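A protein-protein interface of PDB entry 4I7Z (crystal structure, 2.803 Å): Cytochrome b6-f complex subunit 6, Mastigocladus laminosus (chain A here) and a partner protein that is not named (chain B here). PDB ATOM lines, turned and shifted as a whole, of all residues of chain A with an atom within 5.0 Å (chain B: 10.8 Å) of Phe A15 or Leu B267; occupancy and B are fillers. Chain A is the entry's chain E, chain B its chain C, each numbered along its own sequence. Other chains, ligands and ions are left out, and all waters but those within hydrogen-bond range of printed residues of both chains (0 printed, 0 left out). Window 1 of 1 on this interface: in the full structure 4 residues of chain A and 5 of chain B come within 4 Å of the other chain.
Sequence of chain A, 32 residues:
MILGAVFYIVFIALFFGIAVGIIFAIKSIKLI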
ATOM      1  N   VAL A  10       9.797 -19.173  -9.774  1.00  0.00           N
ATOM      2  CA  VAL A  10       9.531 -18.721 -11.140  1.00  0.00           C
ATOM      3  C   VAL A  10      10.691 -19.060 -12.085  1.00  0.00           C
ATOM      4  O   VAL A  10      10.471 -19.432 -13.239  1.00  0.00           O
ATOM      5  CB  VAL A  10       9.245 -17.199 -11.188  1.00  0.00           C
ATOM      6  CG1 VAL A  10       9.087 -16.712 -12.632  1.00  0.00           C
ATOM      7  CG2 VAL A  10       7.997 -16.867 -10.377  1.00  0.00           C
ATOM      8  N   PHE A  11      11.917 -18.926 -11.587  1.00  0.00           N
ATOM      9  CA  PHE A  11      13.128 -19.203 -12.366  1.00  0.00           C
ATOM     10  C   PHE A  11      13.196 -20.678 -12.768  1.00  0.00           C
ATOM     11  O   PHE A  11      13.262 -21.021 -13.967  1.00  0.00           O
ATOM     12  CB  PHE A  11      14.360 -18.847 -11.524  1.00  0.00           C
ATOM     13  CG  PHE A  11      15.521 -18.305 -12.314  1.00  0.00           C
ATOM     14  CD1 PHE A  11      16.341 -17.330 -11.764  1.00  0.00           C
ATOM     15  CD2 PHE A  11      15.813 -18.779 -13.581  1.00  0.00           C
ATOM     16  CE1 PHE A  11      17.421 -16.829 -12.466  1.00  0.00           C
ATOM     17  CE2 PHE A  11      16.894 -18.277 -14.291  1.00  0.00           C
ATOM     18  CZ  PHE A  11      17.699 -17.302 -13.733  1.00  0.00           C
ATOM     19  N   ILE A  12      13.179 -21.554 -11.765  1.00  0.00           N
ATOM     20  CA  ILE A  12      13.256 -22.981 -12.038  1.00  0.00           C
ATOM     21  C   ILE A  12      12.031 -23.425 -12.826  1.00  0.00           C
ATOM     22  O   ILE A  12      12.150 -24.222 -13.747  1.00  0.00           O
ATOM     23  CB  ILE A  12      13.416 -23.820 -10.754  1.00  0.00           C
ATOM     24  CG1 ILE A  12      14.738 -23.463 -10.079  1.00  0.00           C
ATOM     25  CG2 ILE A  12      13.391 -25.316 -11.079  1.00  0.00           C
ATOM     26  CD1 ILE A  12      15.094 -24.320  -8.892  1.00  0.00           C
ATOM     27  N   ALA A  13      10.862 -22.901 -12.476  1.00  0.00           N
ATOM     28  CA  ALA A  13       9.645 -23.245 -13.202  1.00  0.00           C
ATOM     29  C   ALA A  13       9.797 -22.857 -14.668  1.00  0.00           C
ATOM     30  O   ALA A  13       9.445 -23.627 -15.560  1.00  0.00           O
ATOM     31  CB  ALA A  13       8.434 -22.558 -12.588  1.00  0.00           C
ATOM     32  N   LEU A  14      10.335 -21.664 -14.909  1.00  0.00           N
ATOM     33  CA  LEU A  14      10.565 -21.190 -16.270  1.00  0.00           C
ATOM     34  C   LEU A  14      11.458 -22.145 -17.045  1.00  0.00           C
ATOM     35  O   LEU A  14      11.077 -22.630 -18.111  1.00  0.00           O
ATOM     36  CB  LEU A  14      11.194 -19.799 -16.256  1.00  0.00           C
ATOM     37  CG  LEU A  14      10.221 -18.626 -16.321  1.00  0.00           C
ATOM     38  CD1 LEU A  14      10.909 -17.347 -15.902  1.00  0.00           C
ATOM     39  CD2 LEU A  14       9.677 -18.493 -17.728  1.00  0.00           C
ATOM     40  N   PHE A  15      12.644 -22.424 -16.511  1.00  0.00           N
ATOM     41  CA  PHE A  15      13.574 -23.307 -17.222  1.00  0.00           C
ATOM     42  C   PHE A  15      13.097 -24.768 -17.298  1.00  0.00           C
ATOM     43  O   PHE A  15      13.413 -25.488 -18.250  1.00  0.00           O
ATOM     44  CB  PHE A  15      14.971 -23.216 -16.612  1.00  0.00           C
ATOM     45  CG  PHE A  15      15.815 -22.131 -17.215  1.00  0.00           C
ATOM     46  CD1 PHE A  15      15.740 -20.834 -16.744  1.00  0.00           C
ATOM     47  CD2 PHE A  15      16.673 -22.412 -18.266  1.00  0.00           C
ATOM     48  CE1 PHE A  15      16.511 -19.839 -17.304  1.00  0.00           C
ATOM     49  CE2 PHE A  15      17.447 -21.420 -18.832  1.00  0.00           C
ATOM     50  CZ  PHE A  15      17.366 -20.131 -18.352  1.00  0.00           C
ATOM     51  N   PHE A  16      12.328 -25.192 -16.303  1.00  0.00           N
ATOM     52  CA  PHE A  16      11.734 -26.521 -16.305  1.00  0.00           C
ATOM     53  C   PHE A  16      10.741 -26.586 -17.452  1.00  0.00           C
ATOM     54  O   PHE A  16      10.724 -27.544 -18.230  1.00  0.00           O
ATOM     55  CB  PHE A  16      11.026 -26.786 -14.975  1.00  0.00           C
ATOM     56  CG  PHE A  16      10.522 -28.191 -14.822  1.00  0.00           C
ATOM     57  CD1 PHE A  16       9.293 -28.564 -15.343  1.00  0.00           C
ATOM     58  CD2 PHE A  16      11.273 -29.138 -14.150  1.00  0.00           C
ATOM     59  CE1 PHE A  16       8.827 -29.861 -15.202  1.00  0.00           C
ATOM     60  CE2 PHE A  16      10.812 -30.432 -14.004  1.00  0.00           C
ATOM     61  CZ  PHE A  16       9.588 -30.795 -14.532  1.00  0.00           C
ATOM     62  N   GLY A  17       9.918 -25.546 -17.553  1.00  0.00           N
ATOM     63  CA  GLY A  17       8.949 -25.427 -18.625  1.00  0.00           C
ATOM     64  C   GLY A  17       9.636 -25.428 -19.975  1.00  0.00           C
ATOM     65  O   GLY A  17       9.196 -26.112 -20.899  1.00  0.00           O
ATOM     66  N   ILE A  18      10.720 -24.664 -20.084  1.00  0.00           N
ATOM     67  CA  ILE A  18      11.532 -24.663 -21.299  1.00  0.00           C
ATOM     68  C   ILE A  18      12.027 -26.076 -21.620  1.00  0.00           C
ATOM     69  O   ILE A  18      11.951 -26.511 -22.765  1.00  0.00           O
ATOM     70  CB  ILE A  18      12.733 -23.686 -21.190  1.00  0.00           C
ATOM     71  CG1 ILE A  18      12.238 -22.246 -21.113  1.00  0.00           C
ATOM     72  CG2 ILE A  18      13.669 -23.817 -22.394  1.00  0.00           C
ATOM     73  CD1 ILE A  18      13.312 -21.262 -20.747  1.00  0.00           C
ATOM     74  N   ALA A  19      12.528 -26.794 -20.619  1.00  0.00           N
ATOM     75  CA  ALA A  19      12.974 -28.172 -20.834  1.00  0.00           C
ATOM     76  C   ALA A  19      11.853 -29.074 -21.354  1.00  0.00           C
ATOM     77  O   ALA A  19      11.963 -29.666 -22.437  1.00  0.00           O
ATOM     78  CB  ALA A  19      13.554 -28.745 -19.552  1.00  0.00           C
ATOM     79  N   MET B 258      26.030 -11.270 -14.999  1.00  0.00           N
ATOM     80  CA  MET B 258      26.235 -12.580 -14.405  1.00  0.00           C
ATOM     81  C   MET B 258      24.985 -13.429 -14.633  1.00  0.00           C
ATOM     82  O   MET B 258      25.077 -14.568 -15.115  1.00  0.00           O
ATOM     83  CB  MET B 258      26.557 -12.446 -12.910  1.00  0.00           C
ATOM     84  CG  MET B 258      26.832 -13.764 -12.186  1.00  0.00           C
ATOM     85  SD  MET B 258      25.349 -14.520 -11.490  1.00  0.00           S
ATOM     86  CE  MET B 258      24.940 -13.384 -10.166  1.00  0.00           C
ATOM     87  N   ILE B 259      23.823 -12.862 -14.319  1.00  0.00           N
ATOM     88  CA  ILE B 259      22.560 -13.571 -14.508  1.00  0.00           C
ATOM     89  C   ILE B 259      22.422 -14.064 -15.947  1.00  0.00           C
ATOM     90  O   ILE B 259      22.090 -15.236 -16.192  1.00  0.00           O
ATOM     91  CB  ILE B 259      21.363 -12.686 -14.155  1.00  0.00           C
ATOM     92  CG1 ILE B 259      21.391 -12.351 -12.665  1.00  0.00           C
ATOM     93  CG2 ILE B 259      20.050 -13.397 -14.502  1.00  0.00           C
ATOM     94  CD1 ILE B 259      20.386 -11.299 -12.243  1.00  0.00           C
ATOM     95  N   ALA B 260      22.687 -13.169 -16.893  1.00  0.00           N
ATOM     96  CA  ALA B 260      22.663 -13.545 -18.302  1.00  0.00           C
ATOM     97  C   ALA B 260      23.550 -14.763 -18.563  1.00  0.00           C
ATOM     98  O   ALA B 260      23.100 -15.759 -19.143  1.00  0.00           O
ATOM     99  CB  ALA B 260      23.110 -12.387 -19.152  1.00  0.00           C
ATOM    100  N   PHE B 261      24.802 -14.673 -18.122  1.00  0.00           N
ATOM    101  CA  PHE B 261      25.759 -15.767 -18.293  1.00  0.00           C
ATOM    102  C   PHE B 261      25.212 -17.087 -17.747  1.00  0.00           C
ATOM    103  O   PHE B 261      25.230 -18.110 -18.439  1.00  0.00           O
ATOM    104  CB  PHE B 261      27.084 -15.424 -17.601  1.00  0.00           C
ATOM    105  CG  PHE B 261      28.160 -16.466 -17.783  1.00  0.00           C
ATOM    106  CD1 PHE B 261      28.486 -17.335 -16.752  1.00  0.00           C
ATOM    107  CD2 PHE B 261      28.849 -16.573 -18.980  1.00  0.00           C
ATOM    108  CE1 PHE B 261      29.477 -18.291 -16.917  1.00  0.00           C
ATOM    109  CE2 PHE B 261      29.838 -17.527 -19.148  1.00  0.00           C
ATOM    110  CZ  PHE B 261      30.151 -18.386 -18.116  1.00  0.00           C
ATOM    111  N   ILE B 262      24.723 -17.053 -16.509  1.00  0.00           N
ATOM    112  CA  ILE B 262      24.146 -18.238 -15.875  1.00  0.00           C
ATOM    113  C   ILE B 262      23.047 -18.835 -16.740  1.00  0.00           C
ATOM    114  O   ILE B 262      23.034 -20.042 -16.997  1.00  0.00           O
ATOM    115  CB  ILE B 262      23.595 -17.907 -14.467  1.00  0.00           C
ATOM    116  CG1 ILE B 262      24.655 -18.200 -13.406  1.00  0.00           C
ATOM    117  CG2 ILE B 262      22.334 -18.718 -14.143  1.00  0.00           C
ATOM    118  CD1 ILE B 262      25.937 -17.440 -13.590  1.00  0.00           C
ATOM    119  N   CYS B 263      22.126 -17.985 -17.189  1.00  0.00           N
ATOM    120  CA  CYS B 263      21.059 -18.442 -18.077  1.00  0.00           C
ATOM    121  C   CYS B 263      21.609 -19.132 -19.325  1.00  0.00           C
ATOM    122  O   CYS B 263      21.148 -20.217 -19.703  1.00  0.00           O
ATOM    123  CB  CYS B 263      20.158 -17.278 -18.477  1.00  0.00           C
ATOM    124  SG  CYS B 263      19.074 -16.719 -17.151  1.00  0.00           S
ATOM    125  N   LEU B 264      22.595 -18.505 -19.958  1.00  0.00           N
ATOM    126  CA  LEU B 264      23.274 -19.124 -21.093  1.00  0.00           C
ATOM    127  C   LEU B 264      23.819 -20.508 -20.731  1.00  0.00           C
ATOM    128  O   LEU B 264      23.617 -21.476 -21.467  1.00  0.00           O
ATOM    129  CB  LEU B 264      24.420 -18.235 -21.567  1.00  0.00           C
ATOM    130  CG  LEU B 264      24.613 -18.110 -23.077  1.00  0.00           C
ATOM    131  CD1 LEU B 264      25.941 -17.435 -23.355  1.00  0.00           C
ATOM    132  CD2 LEU B 264      24.546 -19.450 -23.781  1.00  0.00           C
ATOM    133  N   VAL B 265      24.509 -20.596 -19.598  1.00  0.00           N
ATOM    134  CA  VAL B 265      25.065 -21.867 -19.141  1.00  0.00           C
ATOM    135  C   VAL B 265      23.969 -22.923 -19.027  1.00  0.00           C
ATOM    136  O   VAL B 265      24.101 -24.020 -19.571  1.00  0.00           O
ATOM    137  CB  VAL B 265      25.790 -21.729 -17.773  1.00  0.00           C
ATOM    138  CG1 VAL B 265      26.117 -23.097 -17.190  1.00  0.00           C
ATOM    139  CG2 VAL B 265      27.065 -20.911 -17.916  1.00  0.00           C
ATOM    140  N   MET B 266      22.893 -22.591 -18.321  1.00  0.00           N
ATOM    141  CA  MET B 266      21.789 -23.534 -18.138  1.00  0.00           C
ATOM    142  C   MET B 266      21.201 -23.982 -19.477  1.00  0.00           C
ATOM    143  O   MET B 266      20.924 -25.169 -19.680  1.00  0.00           O
ATOM    144  CB  MET B 266      20.707 -22.921 -17.249  1.00  0.00           C
ATOM    145  CG  MET B 266      21.195 -22.623 -15.831  1.00  0.00           C
ATOM    146  SD  MET B 266      19.912 -22.109 -14.670  1.00  0.00           S
ATOM    147  CE  MET B 266      19.303 -20.629 -15.456  1.00  0.00           C
ATOM    148  N   LEU B 267      21.025 -23.033 -20.389  1.00  0.00           N
ATOM    149  CA  LEU B 267      20.585 -23.349 -21.741  1.00  0.00           C
ATOM    150  C   LEU B 267      21.511 -24.385 -22.376  1.00  0.00           C
ATOM    151  O   LEU B 267      21.061 -25.432 -22.856  1.00  0.00           O
ATOM    152  CB  LEU B 267      20.567 -22.079 -22.596  1.00  0.00           C
ATOM    153  CG  LEU B 267      19.328 -21.854 -23.467  1.00  0.00           C
ATOM    154  CD1 LEU B 267      19.087 -23.039 -24.404  1.00  0.00           C
ATOM    155  CD2 LEU B 267      18.108 -21.583 -22.595  1.00  0.00           C
ATOM    156  N   ALA B 268      22.808 -24.090 -22.367  1.00  0.00           N
ATOM    157  CA  ALA B 268      23.799 -24.986 -22.963  1.00  0.00           C
ATOM    158  C   ALA B 268      23.754 -26.386 -22.348  1.00  0.00           C
ATOM    159  O   ALA B 268      23.751 -27.398 -23.062  1.00  0.00           O
ATOM    160  CB  ALA B 268      25.193 -24.391 -22.824  1.00  0.00           C
ATOM    161  N   GLN B 269      23.718 -26.437 -21.023  1.00  0.00           N
ATOM    162  CA  GLN B 269      23.620 -27.703 -20.313  1.00  0.00           C
ATOM    163  C   GLN B 269      22.417 -28.489 -20.809  1.00  0.00           C
ATOM    164  O   GLN B 269      22.522 -29.672 -21.182  1.00  0.00           O
ATOM    165  CB  GLN B 269      23.493 -27.452 -18.810  1.00  0.00           C
ATOM    166  CG  GLN B 269      24.749 -26.874 -18.192  1.00  0.00           C
ATOM    167  CD  GLN B 269      24.572 -26.505 -16.734  1.00  0.00           C
ATOM    168  OE1 GLN B 269      23.609 -25.833 -16.364  1.00  0.00           O
ATOM    169  NE2 GLN B 269      25.508 -26.936 -15.897  1.00  0.00           N
ATOM    170  N   LEU B 270      21.274 -27.814 -20.818  1.00  0.00           N
ATOM    171  CA  LEU B 270      20.037 -28.420 -21.279  1.00  0.00           C
ATOM    172  C   LEU B 270      20.201 -28.999 -22.680  1.00  0.00           C
ATOM    173  O   LEU B 270      19.868 -30.165 -22.921  1.00  0.00           O
ATOM    174  CB  LEU B 270      18.914 -27.387 -21.252  1.00  0.00           C
ATOM    175  CG  LEU B 270      17.535 -27.886 -21.673  1.00  0.00           C
ATOM    176  CD1 LEU B 270      16.470 -27.305 -20.774  1.00  0.00           C
ATOM    177  CD2 LEU B 270      17.261 -27.514 -23.118  1.00  0.00           C
ATOM    178  N   MET B 271      20.732 -28.201 -23.600  1.00  0.00           N
ATOM    179  CA  MET B 271      20.918 -28.683 -24.965  1.00  0.00           C
ATOM    180  C   MET B 271      21.825 -29.912 -25.014  1.00  0.00           C
ATOM    181  O   MET B 271      21.526 -30.871 -25.725  1.00  0.00           O
ATOM    182  CB  MET B 271      21.453 -27.578 -25.881  1.00  0.00           C
ATOM    183  CG  MET B 271      20.389 -26.968 -26.797  1.00  0.00           C
ATOM    184  SD  MET B 271      18.854 -26.610 -25.921  1.00  0.00           S
ATOM    185  CE  MET B 271      17.906 -25.732 -27.160  1.00  0.00           C
ATOM    186  N   LEU B 272      22.919 -29.896 -24.258  1.00  0.00           N
ATOM    187  CA  LEU B 272      23.802 -31.066 -24.191  1.00  0.00           C
ATOM    188  C   LEU B 272      23.069 -32.329 -23.725  1.00  0.00           C
ATOM    189  O   LEU B 272      23.187 -33.400 -24.342  1.00  0.00           O
ATOM    190  CB  LEU B 272      24.985 -30.790 -23.266  1.00  0.00           C
ATOM    191  CG  LEU B 272      26.056 -29.866 -23.847  1.00  0.00           C
ATOM    192  CD1 LEU B 272      27.013 -29.420 -22.761  1.00  0.00           C
ATOM    193  CD2 LEU B 272      26.813 -30.550 -24.978  1.00  0.00           C
ATOM    194  N   ILE B 273      22.316 -32.207 -22.634  1.00  0.00           N
ATOM    195  CA  ILE B 273      21.530 -33.338 -22.140  1.00  0.00           C
ATOM    196  C   ILE B 273      20.521 -33.820 -23.187  1.00  0.00           C
ATOM    197  O   ILE B 273      20.342 -35.027 -23.380  1.00  0.00           O
ATOM    198  CB  ILE B 273      20.779 -32.985 -20.837  1.00  0.00           C
ATOM    199  CG1 ILE B 273      21.761 -32.587 -19.733  1.00  0.00           C
ATOM    200  CG2 ILE B 273      19.919 -34.155 -20.364  1.00  0.00           C
ATOM    201  CD1 ILE B 273      22.836 -33.602 -19.446  1.00  0.00           C
ATOM    202  N   LEU B 274      19.855 -32.881 -23.853  1.00  0.00           N
ATOM    203  CA  LEU B 274      18.931 -33.243 -24.923  1.00  0.00           C
ATOM    204  C   LEU B 274      19.648 -34.030 -26.006  1.00  0.00           C
ATOM    205  O   LEU B 274      19.162 -35.071 -26.449  1.00  0.00           O
ATOM    206  CB  LEU B 274      18.287 -32.002 -25.533  1.00  0.00           C
ATOM    207  CG  LEU B 274      17.257 -31.307 -24.648  1.00  0.00           C
ATOM    208  CD1 LEU B 274      16.886 -29.988 -25.271  1.00  0.00           C
ATOM    209  CD2 LEU B 274      16.018 -32.170 -24.456  1.00  0.00           C
ATOM    210  N   LYS B 275      20.807 -33.533 -26.428  1.00  0.00           N
ATOM    211  CA  LYS B 275      21.606 -34.245 -27.414  1.00  0.00           C
ATOM    212  C   LYS B 275      21.891 -35.670 -26.945  1.00  0.00           C
ATOM    213  O   LYS B 275      21.690 -36.624 -27.701  1.00  0.00           O
ATOM    214  CB  LYS B 275      22.917 -33.512 -27.694  1.00  0.00           C
ATOM    215  CG  LYS B 275      23.858 -34.255 -28.639  1.00  0.00           C
ATOM    216  CD  LYS B 275      23.262 -34.425 -30.030  1.00  0.00           C
ATOM    217  CE  LYS B 275      24.049 -35.434 -30.849  1.00  0.00           C
ATOM    218  NZ  LYS B 275      23.743 -35.339 -32.302  1.00  0.00           N
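Printed residues of chain B within 4 Å of Phe A15: Cys B263 (3.99 Å), Met B266 (3.4 Å) and Leu B267 (3.8 Å).
Of chain A, only Phe A15 (3.8 Å) comes within 4 Å of Leu B267.
No residue of chain B comes within 4 Å of Leu A14.
No residue of chain B comes within 4 Å of Gly A17.
No residue of chain B comes within 4 Å of Ile A18.
Of the printed residues of chain A, Cys B263 touches Phe A11 and Phe A15.
Of the printed residues of chain A, Leu B270 touches Ala A19.
Printed residues of chain A within 4 Å of Met B266: Phe A11 (3.6 Å) and Phe A15 (3.4 Å).
The nearest printed residue of chain B that does not touch Phe A15 is Leu B270 (4.4 Å).
The nearest printed residue of chain A that does not touch Leu B267 is Ile A18 (5.0 Å).
The nearest printed residue of chain A that does not touch Cys B263 is Ile A18 (8.0 Å).
O of Ile B259 sits at hydrogen-bond distance from SG of Cys B263.
Of the 18 printed residues of chain B, 4 touch a printed residue of chain A.
Hydrophobic or aromatic side chains of chain B within 4 Å of the printed part of chain A: Met B266, Leu B267 and Leu B270.
Of the 10 printed residues of chain A, 3 touch a printed residue of chain B.
Along chain A the printed residues that touch a printed residue of chain B span positions 11 to 19.
Phe A11 touches Cys B263.
CE of Met B266 touches CE2 of Phe A11 (3.6 Å).
Phe A15 touches Cys B263.
Phe A15 touches Met B266.
CD2 of Leu B267 touches CE2 of Phe A15, 3.8 Å away.
Ala A19 touches Leu B270.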
